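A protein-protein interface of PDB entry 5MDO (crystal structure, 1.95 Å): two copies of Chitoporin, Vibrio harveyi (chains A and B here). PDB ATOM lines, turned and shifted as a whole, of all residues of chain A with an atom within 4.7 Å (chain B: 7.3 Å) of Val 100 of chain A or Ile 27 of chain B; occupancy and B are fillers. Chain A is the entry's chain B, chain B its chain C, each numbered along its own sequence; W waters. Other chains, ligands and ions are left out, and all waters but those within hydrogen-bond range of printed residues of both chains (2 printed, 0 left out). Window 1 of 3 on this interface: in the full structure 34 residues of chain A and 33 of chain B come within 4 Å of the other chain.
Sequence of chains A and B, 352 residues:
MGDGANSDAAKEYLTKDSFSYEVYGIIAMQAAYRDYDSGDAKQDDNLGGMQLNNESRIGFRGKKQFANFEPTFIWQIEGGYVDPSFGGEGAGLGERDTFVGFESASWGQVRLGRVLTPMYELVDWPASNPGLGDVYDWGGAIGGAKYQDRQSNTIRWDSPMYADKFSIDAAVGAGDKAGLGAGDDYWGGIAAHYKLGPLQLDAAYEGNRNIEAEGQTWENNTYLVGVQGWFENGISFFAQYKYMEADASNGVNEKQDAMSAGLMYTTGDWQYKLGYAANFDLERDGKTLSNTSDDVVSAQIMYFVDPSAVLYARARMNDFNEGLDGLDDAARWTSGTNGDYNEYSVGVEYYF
O of Met 29 of chain B sits at hydrogen-bond distance from N of Val 348 of chain B.
The chain-end carboxylate (OXT) of Phe 352 of chain B sits at hydrogen-bond distance from the backbone NH (N) of Gly 25 of chain B (3.0 Å).
N of Ile 27 of chain B lies within hydrogen-bond range of O of Tyr 350 of chain B (2.7 Å).
N of Leu 112 of chain A lies within hydrogen-bond range of O of Val 100 of chain A (2.8 Å).
The side-chain hydroxyl (OG) of Ser 56 of chain B lies within hydrogen-bond range of the side-chain amide oxygen (OD1) of Asn 54 of chain B (2.6 Å).
N of Ala 28 of chain B is in hydrogen-bond range of OG of Ser 56 of chain B, 3.0 Å away.
CZ of Phe 73 of chain A touches CG2 of Ile 27 of chain B (3.8 Å).
CD2 of Tyr 350 of chain B touches CE2 of Phe 73 of chain A, at 3.8 Å.
Trp 75 of chain A touches Ile 27 of chain B (CE3 to CD1, 3.7 Å).
Trp 75 of chain A touches Tyr 350 of chain B.
Ile 77 of chain A touches Ile 27 of chain B (CD1 to CD1, 3.98 Å).
Ser 56 of chain B touches Ile 77 of chain A (CB to CD1, 3.997 Å).
CG1 of Ile 58 of chain B touches CD1 of Ile 77 of chain A, at 3.8 Å.
CG1 of Val 100 of chain A touches CG2 of Ile 27 of chain B, 3.5 Å away.
CG2 of Val 100 of chain A touches CB of Met 29 of chain B, at 3.6 Å.
CE of Met 29 of chain B touches O of Leu 112 of chain A, at 3.3 Å.
Val 100 of chain A touches just these residues of chain B: Ile 27 (3.5 Å) and Met 29 (3.6 Å).
Printed residues of chain A within 4 Å of Ile 27 of chain B: Phe 73 (3.8 Å), Trp 75 (3.7 Å), Ile 77 (3.98 Å) and Val 100 (3.5 Å).
Printed residues of chain A within 4 Å of Ile 58 of chain B: Ile 77.
Of the printed residues of chain A, Ser 56 of chain B touches Ile 77 (3.997 Å).
Printed residues of chain B within 4 Å of Phe 73 of chain A: Ile 27 (3.8 Å) and Tyr 350 (3.8 Å).
Of the printed residues of chain A, Met 29 of chain B touches Val 100 and Leu 112.
The nearest printed residue of chain A that does not touch Ile 27 of chain B is Phe 99 of chain A (5.4 Å).
The nearest printed residue of chain A that does not touch Tyr 350 of chain B is Ile 74 of chain A (7.4 Å).
Printed residues of chain A that touch a printed residue of chain B: Phe 73, Trp 75, Ile 77, Val 100 and Leu 112.
Hydrophobic or aromatic side chains of chain A within 4 Å of the printed part of chain B: Phe 73, Trp 75, Ile 77 and Val 100.
Of the 20 printed residues of chain B, 6 touch a printed residue of chain A.
Hydrophobic or aromatic side chains of chain B within 4 Å of the printed part of chain A: Ile 27, Met 29, Ile 58, Tyr 350 and Phe 352.
No position is printed for both chains.
Of the 11 pairs that touch across the chains among the printed residues, none has its exchanged pair printed and touching as well.
Water W2 bridges OH of Tyr 350 of chain B and NE1 of Trp 75 of chain A.
Water W1 lies within hydrogen-bond range of the side-chain amide nitrogen of Asn 54 of chain B (3.1 Å), the side-chain hydroxyl of Ser 56 of chain B (3.2 Å) and the backbone carbonyl oxygen of Phe 99 of chain A (3.2 Å).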
ATOM      1  N   PHE A  73      26.583   8.727  -1.808  1.00  0.00           N
ATOM      2  CA  PHE A  73      26.465   9.472  -3.081  1.00  0.00           C
ATOM      3  C   PHE A  73      27.869   9.606  -3.703  1.00  0.00           C
ATOM      4  O   PHE A  73      28.822   9.945  -3.018  1.00  0.00           O
ATOM      5  CB  PHE A  73      25.851  10.854  -2.813  1.00  0.00           C
ATOM      6  CG  PHE A  73      25.568  11.660  -4.041  1.00  0.00           C
ATOM      7  CD1 PHE A  73      24.642  11.242  -4.951  1.00  0.00           C
ATOM      8  CD2 PHE A  73      26.252  12.850  -4.274  1.00  0.00           C
ATOM      9  CE1 PHE A  73      24.333  12.029  -6.070  1.00  0.00           C
ATOM     10  CE2 PHE A  73      25.971  13.656  -5.398  1.00  0.00           C
ATOM     11  CZ  PHE A  73      24.980  13.225  -6.295  1.00  0.00           C
ATOM     12  N   ILE A  74      27.963   9.392  -4.978  1.00  0.00           N
ATOM     13  CA  ILE A  74      29.196   9.595  -5.755  1.00  0.00           C
ATOM     14  C   ILE A  74      28.942  10.429  -6.996  1.00  0.00           C
ATOM     15  O   ILE A  74      27.826  10.450  -7.535  1.00  0.00           O
ATOM     16  CB  ILE A  74      29.814   8.239  -6.170  1.00  0.00           C
ATOM     17  CG1 ILE A  74      28.914   7.468  -7.127  1.00  0.00           C
ATOM     18  CG2 ILE A  74      30.096   7.402  -4.946  1.00  0.00           C
ATOM     19  CD1 ILE A  74      29.529   6.138  -7.719  1.00  0.00           C
ATOM     20  N   TRP A  75      29.983  11.135  -7.459  1.00  0.00           N
ATOM     21  CA  TRP A  75      29.848  11.942  -8.634  1.00  0.00           C
ATOM     22  C   TRP A  75      31.228  12.154  -9.284  1.00  0.00           C
ATOM     23  O   TRP A  75      32.262  12.074  -8.628  1.00  0.00           O
ATOM     24  CB  TRP A  75      29.153  13.302  -8.339  1.00  0.00           C
ATOM     25  CG  TRP A  75      29.950  14.188  -7.414  1.00  0.00           C
ATOM     26  CD1 TRP A  75      29.886  14.172  -6.040  1.00  0.00           C
ATOM     27  CD2 TRP A  75      30.975  15.130  -7.755  1.00  0.00           C
ATOM     28  NE1 TRP A  75      30.769  15.099  -5.506  1.00  0.00           N
ATOM     29  CE2 TRP A  75      31.491  15.658  -6.534  1.00  0.00           C
ATOM     30  CE3 TRP A  75      31.554  15.539  -8.976  1.00  0.00           C
ATOM     31  CZ2 TRP A  75      32.526  16.573  -6.496  1.00  0.00           C
ATOM     32  CZ3 TRP A  75      32.562  16.490  -8.934  1.00  0.00           C
ATOM     33  CH2 TRP A  75      33.014  17.017  -7.713  1.00  0.00           C
ATOM     34  N   ILE A  77      32.942  14.494 -12.878  1.00  0.00           N
ATOM     35  CA  ILE A  77      32.837  15.289 -14.074  1.00  0.00           C
ATOM     36  C   ILE A  77      34.223  15.294 -14.733  1.00  0.00           C
ATOM     37  O   ILE A  77      35.129  15.886 -14.179  1.00  0.00           O
ATOM     38  CB  ILE A  77      32.407  16.750 -13.750  1.00  0.00           C
ATOM     39  CG1 ILE A  77      31.020  16.801 -13.049  1.00  0.00           C
ATOM     40  CG2 ILE A  77      32.448  17.619 -15.016  1.00  0.00           C
ATOM     41  CD1 ILE A  77      30.692  18.168 -12.431  1.00  0.00           C
ATOM     42  N   PHE A  99      28.969  11.636 -14.262  1.00  0.00           N
ATOM     43  CA  PHE A  99      27.790  10.930 -13.686  1.00  0.00           C
ATOM     44  C   PHE A  99      27.529  11.319 -12.270  1.00  0.00           C
ATOM     45  O   PHE A  99      28.360  11.960 -11.635  1.00  0.00           O
ATOM     46  CB  PHE A  99      28.026   9.359 -13.819  1.00  0.00           C
ATOM     47  CG  PHE A  99      29.277   8.856 -13.141  1.00  0.00           C
ATOM     48  CD1 PHE A  99      29.335   8.683 -11.763  1.00  0.00           C
ATOM     49  CD2 PHE A  99      30.461   8.646 -13.889  1.00  0.00           C
ATOM     50  CE1 PHE A  99      30.539   8.271 -11.152  1.00  0.00           C
ATOM     51  CE2 PHE A  99      31.610   8.143 -13.285  1.00  0.00           C
ATOM     52  CZ  PHE A  99      31.677   7.996 -11.943  1.00  0.00           C
ATOM     53  N   VAL A 100      26.369  10.851 -11.745  1.00  0.00           N
ATOM     54  CA  VAL A 100      26.119  10.810 -10.311  1.00  0.00           C
ATOM     55  C   VAL A 100      25.781   9.369 -10.011  1.00  0.00           C
ATOM     56  O   VAL A 100      25.513   8.584 -10.927  1.00  0.00           O
ATOM     57  CB  VAL A 100      24.952  11.715  -9.855  1.00  0.00           C
ATOM     58  CG1 VAL A 100      25.239  13.113 -10.303  1.00  0.00           C
ATOM     59  CG2 VAL A 100      23.624  11.220 -10.416  1.00  0.00           C
ATOM     60  N   GLY A 101      25.798   8.992  -8.765  1.00  0.00           N
ATOM     61  CA  GLY A 101      25.397   7.613  -8.414  1.00  0.00           C
ATOM     62  C   GLY A 101      25.371   7.352  -6.961  1.00  0.00           C
ATOM     63  O   GLY A 101      25.538   8.270  -6.145  1.00  0.00           O
ATOM     64  N   VAL A 110      25.561   2.056  -8.647  1.00  0.00           N
ATOM     65  CA  VAL A 110      24.725   2.440  -9.768  1.00  0.00           C
ATOM     66  C   VAL A 110      25.074   3.856 -10.170  1.00  0.00           C
ATOM     67  O   VAL A 110      25.205   4.739  -9.279  1.00  0.00           O
ATOM     68  CB  VAL A 110      23.210   2.259  -9.442  1.00  0.00           C
ATOM     69  CG1 VAL A 110      22.790   3.138  -8.301  1.00  0.00           C
ATOM     70  CG2 VAL A 110      22.333   2.629 -10.634  1.00  0.00           C
ATOM     71  N   ARG A 111      25.252   4.067 -11.461  1.00  0.00           N
ATOM     72  CA  ARG A 111      25.607   5.382 -11.991  1.00  0.00           C
ATOM     73  C   ARG A 111      24.573   5.829 -13.017  1.00  0.00           C
ATOM     74  O   ARG A 111      24.046   4.992 -13.795  1.00  0.00           O
ATOM     75  CB  ARG A 111      27.003   5.364 -12.599  1.00  0.00           C
ATOM     76  CG  ARG A 111      28.062   5.190 -11.540  1.00  0.00           C
ATOM     77  CD  ARG A 111      29.437   5.105 -12.210  1.00  0.00           C
ATOM     78  NE  ARG A 111      29.661   3.831 -12.909  1.00  0.00           N
ATOM     79  CZ  ARG A 111      30.558   3.594 -13.878  1.00  0.00           C
ATOM     80  NH1 ARG A 111      31.365   4.562 -14.332  1.00  0.00           N
ATOM     81  NH2 ARG A 111      30.653   2.391 -14.433  1.00  0.00           N
ATOM     82  N   LEU A 112      24.239   7.118 -13.002  1.00  0.00           N
ATOM     83  CA  LEU A 112      23.432   7.746 -14.020  1.00  0.00           C
ATOM     84  C   LEU A 112      24.232   8.819 -14.683  1.00  0.00           C
ATOM     85  O   LEU A 112      24.820   9.700 -13.993  1.00  0.00           O
ATOM     86  CB  LEU A 112      22.193   8.369 -13.411  1.00  0.00           C
ATOM     87  CG  LEU A 112      21.030   7.444 -12.918  1.00  0.00           C
ATOM     88  CD1 LEU A 112      21.584   6.722 -11.774  1.00  0.00           C
ATOM     89  CD2 LEU A 112      19.937   8.345 -12.330  1.00  0.00           C
ATOM     90  N   TYR B  24      33.794  25.418  -6.288  1.00  0.00           N
ATOM     91  CA  TYR B  24      32.466  25.093  -5.769  1.00  0.00           C
ATOM     92  C   TYR B  24      31.720  24.360  -6.873  1.00  0.00           C
ATOM     93  O   TYR B  24      32.131  24.332  -8.047  1.00  0.00           O
ATOM     94  CB  TYR B  24      31.666  26.346  -5.309  1.00  0.00           C
ATOM     95  CG  TYR B  24      31.328  27.295  -6.455  1.00  0.00           C
ATOM     96  CD1 TYR B  24      32.291  28.246  -6.931  1.00  0.00           C
ATOM     97  CD2 TYR B  24      30.087  27.300  -7.032  1.00  0.00           C
ATOM     98  CE1 TYR B  24      31.977  29.122  -7.974  1.00  0.00           C
ATOM     99  CE2 TYR B  24      29.756  28.139  -8.074  1.00  0.00           C
ATOM    100  CZ  TYR B  24      30.733  29.078  -8.553  1.00  0.00           C
ATOM    101  OH  TYR B  24      30.390  29.945  -9.549  1.00  0.00           O
ATOM    102  N   GLY B  25      30.637  23.708  -6.509  1.00  0.00           N
ATOM    103  CA  GLY B  25      29.840  22.971  -7.469  1.00  0.00           C
ATOM    104  C   GLY B  25      28.412  22.738  -7.064  1.00  0.00           C
ATOM    105  O   GLY B  25      28.054  22.828  -5.881  1.00  0.00           O
ATOM    106  N   ILE B  26      27.598  22.495  -8.086  1.00  0.00           N
ATOM    107  CA  ILE B  26      26.245  22.080  -7.907  1.00  0.00           C
ATOM    108  C   ILE B  26      26.166  20.789  -8.718  1.00  0.00           C
ATOM    109  O   ILE B  26      26.397  20.811  -9.931  1.00  0.00           O
ATOM    110  CB  ILE B  26      25.219  23.107  -8.408  1.00  0.00           C
ATOM    111  CG1 ILE B  26      25.233  24.410  -7.526  1.00  0.00           C
ATOM    112  CG2 ILE B  26      23.807  22.526  -8.298  1.00  0.00           C
ATOM    113  CD1 ILE B  26      26.279  25.382  -8.026  1.00  0.00           C
ATOM    114  N   ILE B  27      25.972  19.686  -8.034  1.00  0.00           N
ATOM    115  CA  ILE B  27      25.849  18.368  -8.700  1.00  0.00           C
ATOM    116  C   ILE B  27      24.345  18.082  -8.788  1.00  0.00           C
ATOM    117  O   ILE B  27      23.652  18.028  -7.749  1.00  0.00           O
ATOM    118  CB  ILE B  27      26.560  17.324  -7.895  1.00  0.00           C
ATOM    119  CG1 ILE B  27      28.028  17.659  -7.660  1.00  0.00           C
ATOM    120  CG2 ILE B  27      26.429  15.927  -8.568  1.00  0.00           C
ATOM    121  CD1 ILE B  27      28.808  18.023  -8.925  1.00  0.00           C
ATOM    122  N   ALA B  28      23.809  18.011 -10.004  1.00  0.00           N
ATOM    123  CA  ALA B  28      22.335  17.999 -10.195  1.00  0.00           C
ATOM    124  C   ALA B  28      21.970  17.096 -11.345  1.00  0.00           C
ATOM    125  O   ALA B  28      22.556  17.270 -12.491  1.00  0.00           O
ATOM    126  CB  ALA B  28      21.835  19.400 -10.544  1.00  0.00           C
ATOM    127  N   MET B  29      21.172  16.073 -11.067  1.00  0.00           N
ATOM    128  CA  MET B  29      20.804  15.031 -12.088  1.00  0.00           C
ATOM    129  C   MET B  29      19.334  14.848 -11.978  1.00  0.00           C
ATOM    130  O   MET B  29      18.826  14.609 -10.866  1.00  0.00           O
ATOM    131  CB  MET B  29      21.541  13.727 -11.846  1.00  0.00           C
ATOM    132  CG  MET B  29      21.061  12.541 -12.751  1.00  0.00           C
ATOM    133  SD  MET B  29      21.510  12.937 -14.589  1.00  0.00           S
ATOM    134  CE  MET B  29      23.406  12.642 -14.447  1.00  0.00           C
ATOM    135  N   GLN B  30      18.650  14.980 -13.097  1.00  0.00           N
ATOM    136  CA  GLN B  30      17.211  14.720 -13.192  1.00  0.00           C
ATOM    137  C   GLN B  30      16.951  13.625 -14.267  1.00  0.00           C
ATOM    138  O   GLN B  30      17.495  13.728 -15.391  1.00  0.00           O
ATOM    139  CB  GLN B  30      16.555  16.028 -13.586  1.00  0.00           C
ATOM    140  CG  GLN B  30      15.055  15.910 -13.764  1.00  0.00           C
ATOM    141  CD  GLN B  30      14.477  17.197 -14.288  1.00  0.00           C
ATOM    142  OE1 GLN B  30      15.114  17.931 -15.013  1.00  0.00           O
ATOM    143  NE2 GLN B  30      13.238  17.457 -13.928  1.00  0.00           N
ATOM    144  N   ASN B  54      21.554  16.356 -16.919  1.00  0.00           N
ATOM    145  CA  ASN B  54      22.595  16.547 -15.995  1.00  0.00           C
ATOM    146  C   ASN B  54      22.935  18.069 -16.004  1.00  0.00           C
ATOM    147  O   ASN B  54      23.595  18.559 -16.939  1.00  0.00           O
ATOM    148  CB  ASN B  54      23.858  15.739 -16.376  1.00  0.00           C
ATOM    149  CG  ASN B  54      24.920  15.794 -15.299  1.00  0.00           C
ATOM    150  OD1 ASN B  54      24.913  16.647 -14.372  1.00  0.00           O
ATOM    151  ND2 ASN B  54      25.837  14.917 -15.385  1.00  0.00           N
ATOM    152  N   GLU B  55      22.493  18.765 -14.952  1.00  0.00           N
ATOM    153  CA  GLU B  55      22.743  20.184 -14.753  1.00  0.00           C
ATOM    154  C   GLU B  55      23.916  20.451 -13.826  1.00  0.00           C
ATOM    155  O   GLU B  55      24.076  21.598 -13.312  1.00  0.00           O
ATOM    156  CB  GLU B  55      21.450  20.873 -14.264  1.00  0.00           C
ATOM    157  CG  GLU B  55      20.444  20.859 -15.379  1.00  0.00           C
ATOM    158  CD  GLU B  55      19.087  21.553 -15.007  1.00  0.00           C
ATOM    159  OE1 GLU B  55      18.895  21.745 -13.847  1.00  0.00           O
ATOM    160  OE2 GLU B  55      18.271  21.866 -15.880  1.00  0.00           O
ATOM    161  N   SER B  56      24.735  19.442 -13.582  1.00  0.00           N
ATOM    162  CA  SER B  56      25.917  19.623 -12.782  1.00  0.00           C
ATOM    163  C   SER B  56      26.843  20.722 -13.415  1.00  0.00           C
ATOM    164  O   SER B  56      26.962  20.844 -14.629  1.00  0.00           O
ATOM    165  CB  SER B  56      26.700  18.329 -12.552  1.00  0.00           C
ATOM    166  OG  SER B  56      25.929  17.285 -12.012  1.00  0.00           O
ATOM    167  N   ARG B  57      27.460  21.504 -12.548  1.00  0.00           N
ATOM    168  CA  ARG B  57      28.453  22.520 -12.931  1.00  0.00           C
ATOM    169  C   ARG B  57      29.487  22.770 -11.815  1.00  0.00           C
ATOM    170  O   ARG B  57      29.222  22.616 -10.632  1.00  0.00           O
ATOM    171  CB  ARG B  57      27.784  23.807 -13.357  1.00  0.00           C
ATOM    172  CG  ARG B  57      26.989  24.571 -12.313  1.00  0.00           C
ATOM    173  CD  ARG B  57      25.574  24.252 -12.363  1.00  0.00           C
ATOM    174  NE  ARG B  57      24.714  25.051 -11.538  1.00  0.00           N
ATOM    175  CZ  ARG B  57      23.497  24.718 -11.231  1.00  0.00           C
ATOM    176  NH1 ARG B  57      22.921  23.568 -11.624  1.00  0.00           N
ATOM    177  NH2 ARG B  57      22.821  25.534 -10.457  1.00  0.00           N
ATOM    178  N   ILE B  58      30.694  23.121 -12.254  1.00  0.00           N
ATOM    179  CA  ILE B  58      31.792  23.432 -11.450  1.00  0.00           C
ATOM    180  C   ILE B  58      32.064  24.963 -11.681  1.00  0.00           C
ATOM    181  O   ILE B  58      32.019  25.464 -12.795  1.00  0.00           O
ATOM    182  CB  ILE B  58      32.999  22.690 -11.937  1.00  0.00           C
ATOM    183  CG1 ILE B  58      32.832  21.168 -11.611  1.00  0.00           C
ATOM    184  CG2 ILE B  58      34.272  23.170 -11.281  1.00  0.00           C
ATOM    185  CD1 ILE B  58      32.782  20.788 -10.129  1.00  0.00           C
ATOM    186  N   SER B 308      23.196  19.472   2.799  1.00  0.00           N
ATOM    187  CA  SER B 308      23.703  19.919   1.546  1.00  0.00           C
ATOM    188  C   SER B 308      22.994  19.334   0.269  1.00  0.00           C
ATOM    189  O   SER B 308      23.440  19.570  -0.851  1.00  0.00           O
ATOM    190  CB  SER B 308      25.217  19.753   1.579  1.00  0.00           C
ATOM    191  OG  SER B 308      25.460  18.422   1.141  1.00  0.00           O
ATOM    192  N   ALA B 309      21.879  18.637   0.405  1.00  0.00           N
ATOM    193  CA  ALA B 309      21.289  17.958  -0.754  1.00  0.00           C
ATOM    194  C   ALA B 309      19.823  17.670  -0.632  1.00  0.00           C
ATOM    195  O   ALA B 309      19.311  17.521   0.491  1.00  0.00           O
ATOM    196  CB  ALA B 309      22.027  16.651  -1.014  1.00  0.00           C
ATOM    197  N   VAL B 310      19.165  17.538  -1.778  1.00  0.00           N
ATOM    198  CA  VAL B 310      17.768  17.140  -1.853  1.00  0.00           C
ATOM    199  C   VAL B 310      17.546  16.036  -2.893  1.00  0.00           C
ATOM    200  O   VAL B 310      18.316  15.933  -3.894  1.00  0.00           O
ATOM    201  CB  VAL B 310      16.843  18.318  -2.237  1.00  0.00           C
ATOM    202  CG1 VAL B 310      16.960  19.419  -1.160  1.00  0.00           C
ATOM    203  CG2 VAL B 310      17.157  18.905  -3.568  1.00  0.00           C
ATOM    204  N   VAL B 348      18.144  14.598  -8.039  1.00  0.00           N
ATOM    205  CA  VAL B 348      19.000  14.862  -6.893  1.00  0.00           C
ATOM    206  C   VAL B 348      19.713  16.189  -7.163  1.00  0.00           C
ATOM    207  O   VAL B 348      20.179  16.436  -8.306  1.00  0.00           O
ATOM    208  CB  VAL B 348      19.972  13.693  -6.600  1.00  0.00           C
ATOM    209  CG1 VAL B 348      20.880  13.371  -7.832  1.00  0.00           C
ATOM    210  CG2 VAL B 348      20.876  13.975  -5.388  1.00  0.00           C
ATOM    211  N   GLU B 349      19.859  17.024  -6.133  1.00  0.00           N
ATOM    212  CA  GLU B 349      20.795  18.126  -6.195  1.00  0.00           C
ATOM    213  C   GLU B 349      21.640  18.168  -4.933  1.00  0.00           C
ATOM    214  O   GLU B 349      21.138  17.962  -3.834  1.00  0.00           O
ATOM    215  CB  GLU B 349      20.147  19.480  -6.386  1.00  0.00           C
ATOM    216  CG  GLU B 349      19.215  19.481  -7.508  1.00  0.00           C
ATOM    217  CD  GLU B 349      19.028  20.815  -8.175  1.00  0.00           C
ATOM    218  OE1 GLU B 349      19.377  21.860  -7.577  1.00  0.00           O
ATOM    219  OE2 GLU B 349      18.499  20.758  -9.320  1.00  0.00           O
ATOM    220  N   TYR B 350      22.929  18.465  -5.104  1.00  0.00           N
ATOM    221  CA  TYR B 350      23.898  18.511  -4.021  1.00  0.00           C
ATOM    222  C   TYR B 350      24.826  19.707  -4.245  1.00  0.00           C
ATOM    223  O   TYR B 350      25.294  19.920  -5.383  1.00  0.00           O
ATOM    224  CB  TYR B 350      24.673  17.174  -3.960  1.00  0.00           C
ATOM    225  CG  TYR B 350      25.995  17.165  -3.224  1.00  0.00           C
ATOM    226  CD1 TYR B 350      26.065  17.401  -1.858  1.00  0.00           C
ATOM    227  CD2 TYR B 350      27.183  16.942  -3.895  1.00  0.00           C
ATOM    228  CE1 TYR B 350      27.246  17.365  -1.166  1.00  0.00           C
ATOM    229  CE2 TYR B 350      28.383  16.941  -3.235  1.00  0.00           C
ATOM    230  CZ  TYR B 350      28.432  17.151  -1.873  1.00  0.00           C
ATOM    231  OH  TYR B 350      29.653  17.109  -1.202  1.00  0.00           O
ATOM    232  N   TYR B 351      25.149  20.421  -3.166  1.00  0.00           N
ATOM    233  CA  TYR B 351      25.861  21.711  -3.241  1.00  0.00           C
ATOM    234  C   TYR B 351      27.096  21.578  -2.412  1.00  0.00           C
ATOM    235  O   TYR B 351      27.053  21.099  -1.291  1.00  0.00           O
ATOM    236  CB  TYR B 351      24.995  22.914  -2.709  1.00  0.00           C
ATOM    237  CG  TYR B 351      23.544  22.815  -3.215  1.00  0.00           C
ATOM    238  CD1 TYR B 351      23.140  23.366  -4.444  1.00  0.00           C
ATOM    239  CD2 TYR B 351      22.569  22.111  -2.460  1.00  0.00           C
ATOM    240  CE1 TYR B 351      21.815  23.212  -4.912  1.00  0.00           C
ATOM    241  CE2 TYR B 351      21.244  21.971  -2.915  1.00  0.00           C
ATOM    242  CZ  TYR B 351      20.909  22.494  -4.162  1.00  0.00           C
ATOM    243  OH  TYR B 351      19.599  22.343  -4.604  1.00  0.00           O
ATOM    244  N   PHE B 352      28.235  21.987  -2.972  1.00  0.00           N
ATOM    245  CA  PHE B 352      29.426  22.130  -2.150  1.00  0.00           C
ATOM    246  C   PHE B 352      30.215  23.404  -2.569  1.00  0.00           C
ATOM    247  O   PHE B 352      31.165  23.689  -1.866  1.00  0.00           O
ATOM    248  CB  PHE B 352      30.366  20.894  -2.240  1.00  0.00           C
ATOM    249  CG  PHE B 352      31.022  20.687  -3.581  1.00  0.00           C
ATOM    250  CD1 PHE B 352      30.375  19.980  -4.547  1.00  0.00           C
ATOM    251  CD2 PHE B 352      32.264  21.238  -3.884  1.00  0.00           C
ATOM    252  CE1 PHE B 352      30.935  19.829  -5.792  1.00  0.00           C
ATOM    253  CE2 PHE B 352      32.837  21.061  -5.140  1.00  0.00           C
ATOM    254  CZ  PHE B 352      32.157  20.376  -6.096  1.00  0.00           C
ATOM    255  OXT PHE B 352      29.986  24.068  -3.579  1.00  0.00           O
HETATM  256  O   HOH W   1      27.799  14.857 -12.982  1.00  0.00           O
HETATM  257  O   HOH W   2      31.432  15.633  -2.564  1.00  0.00           O
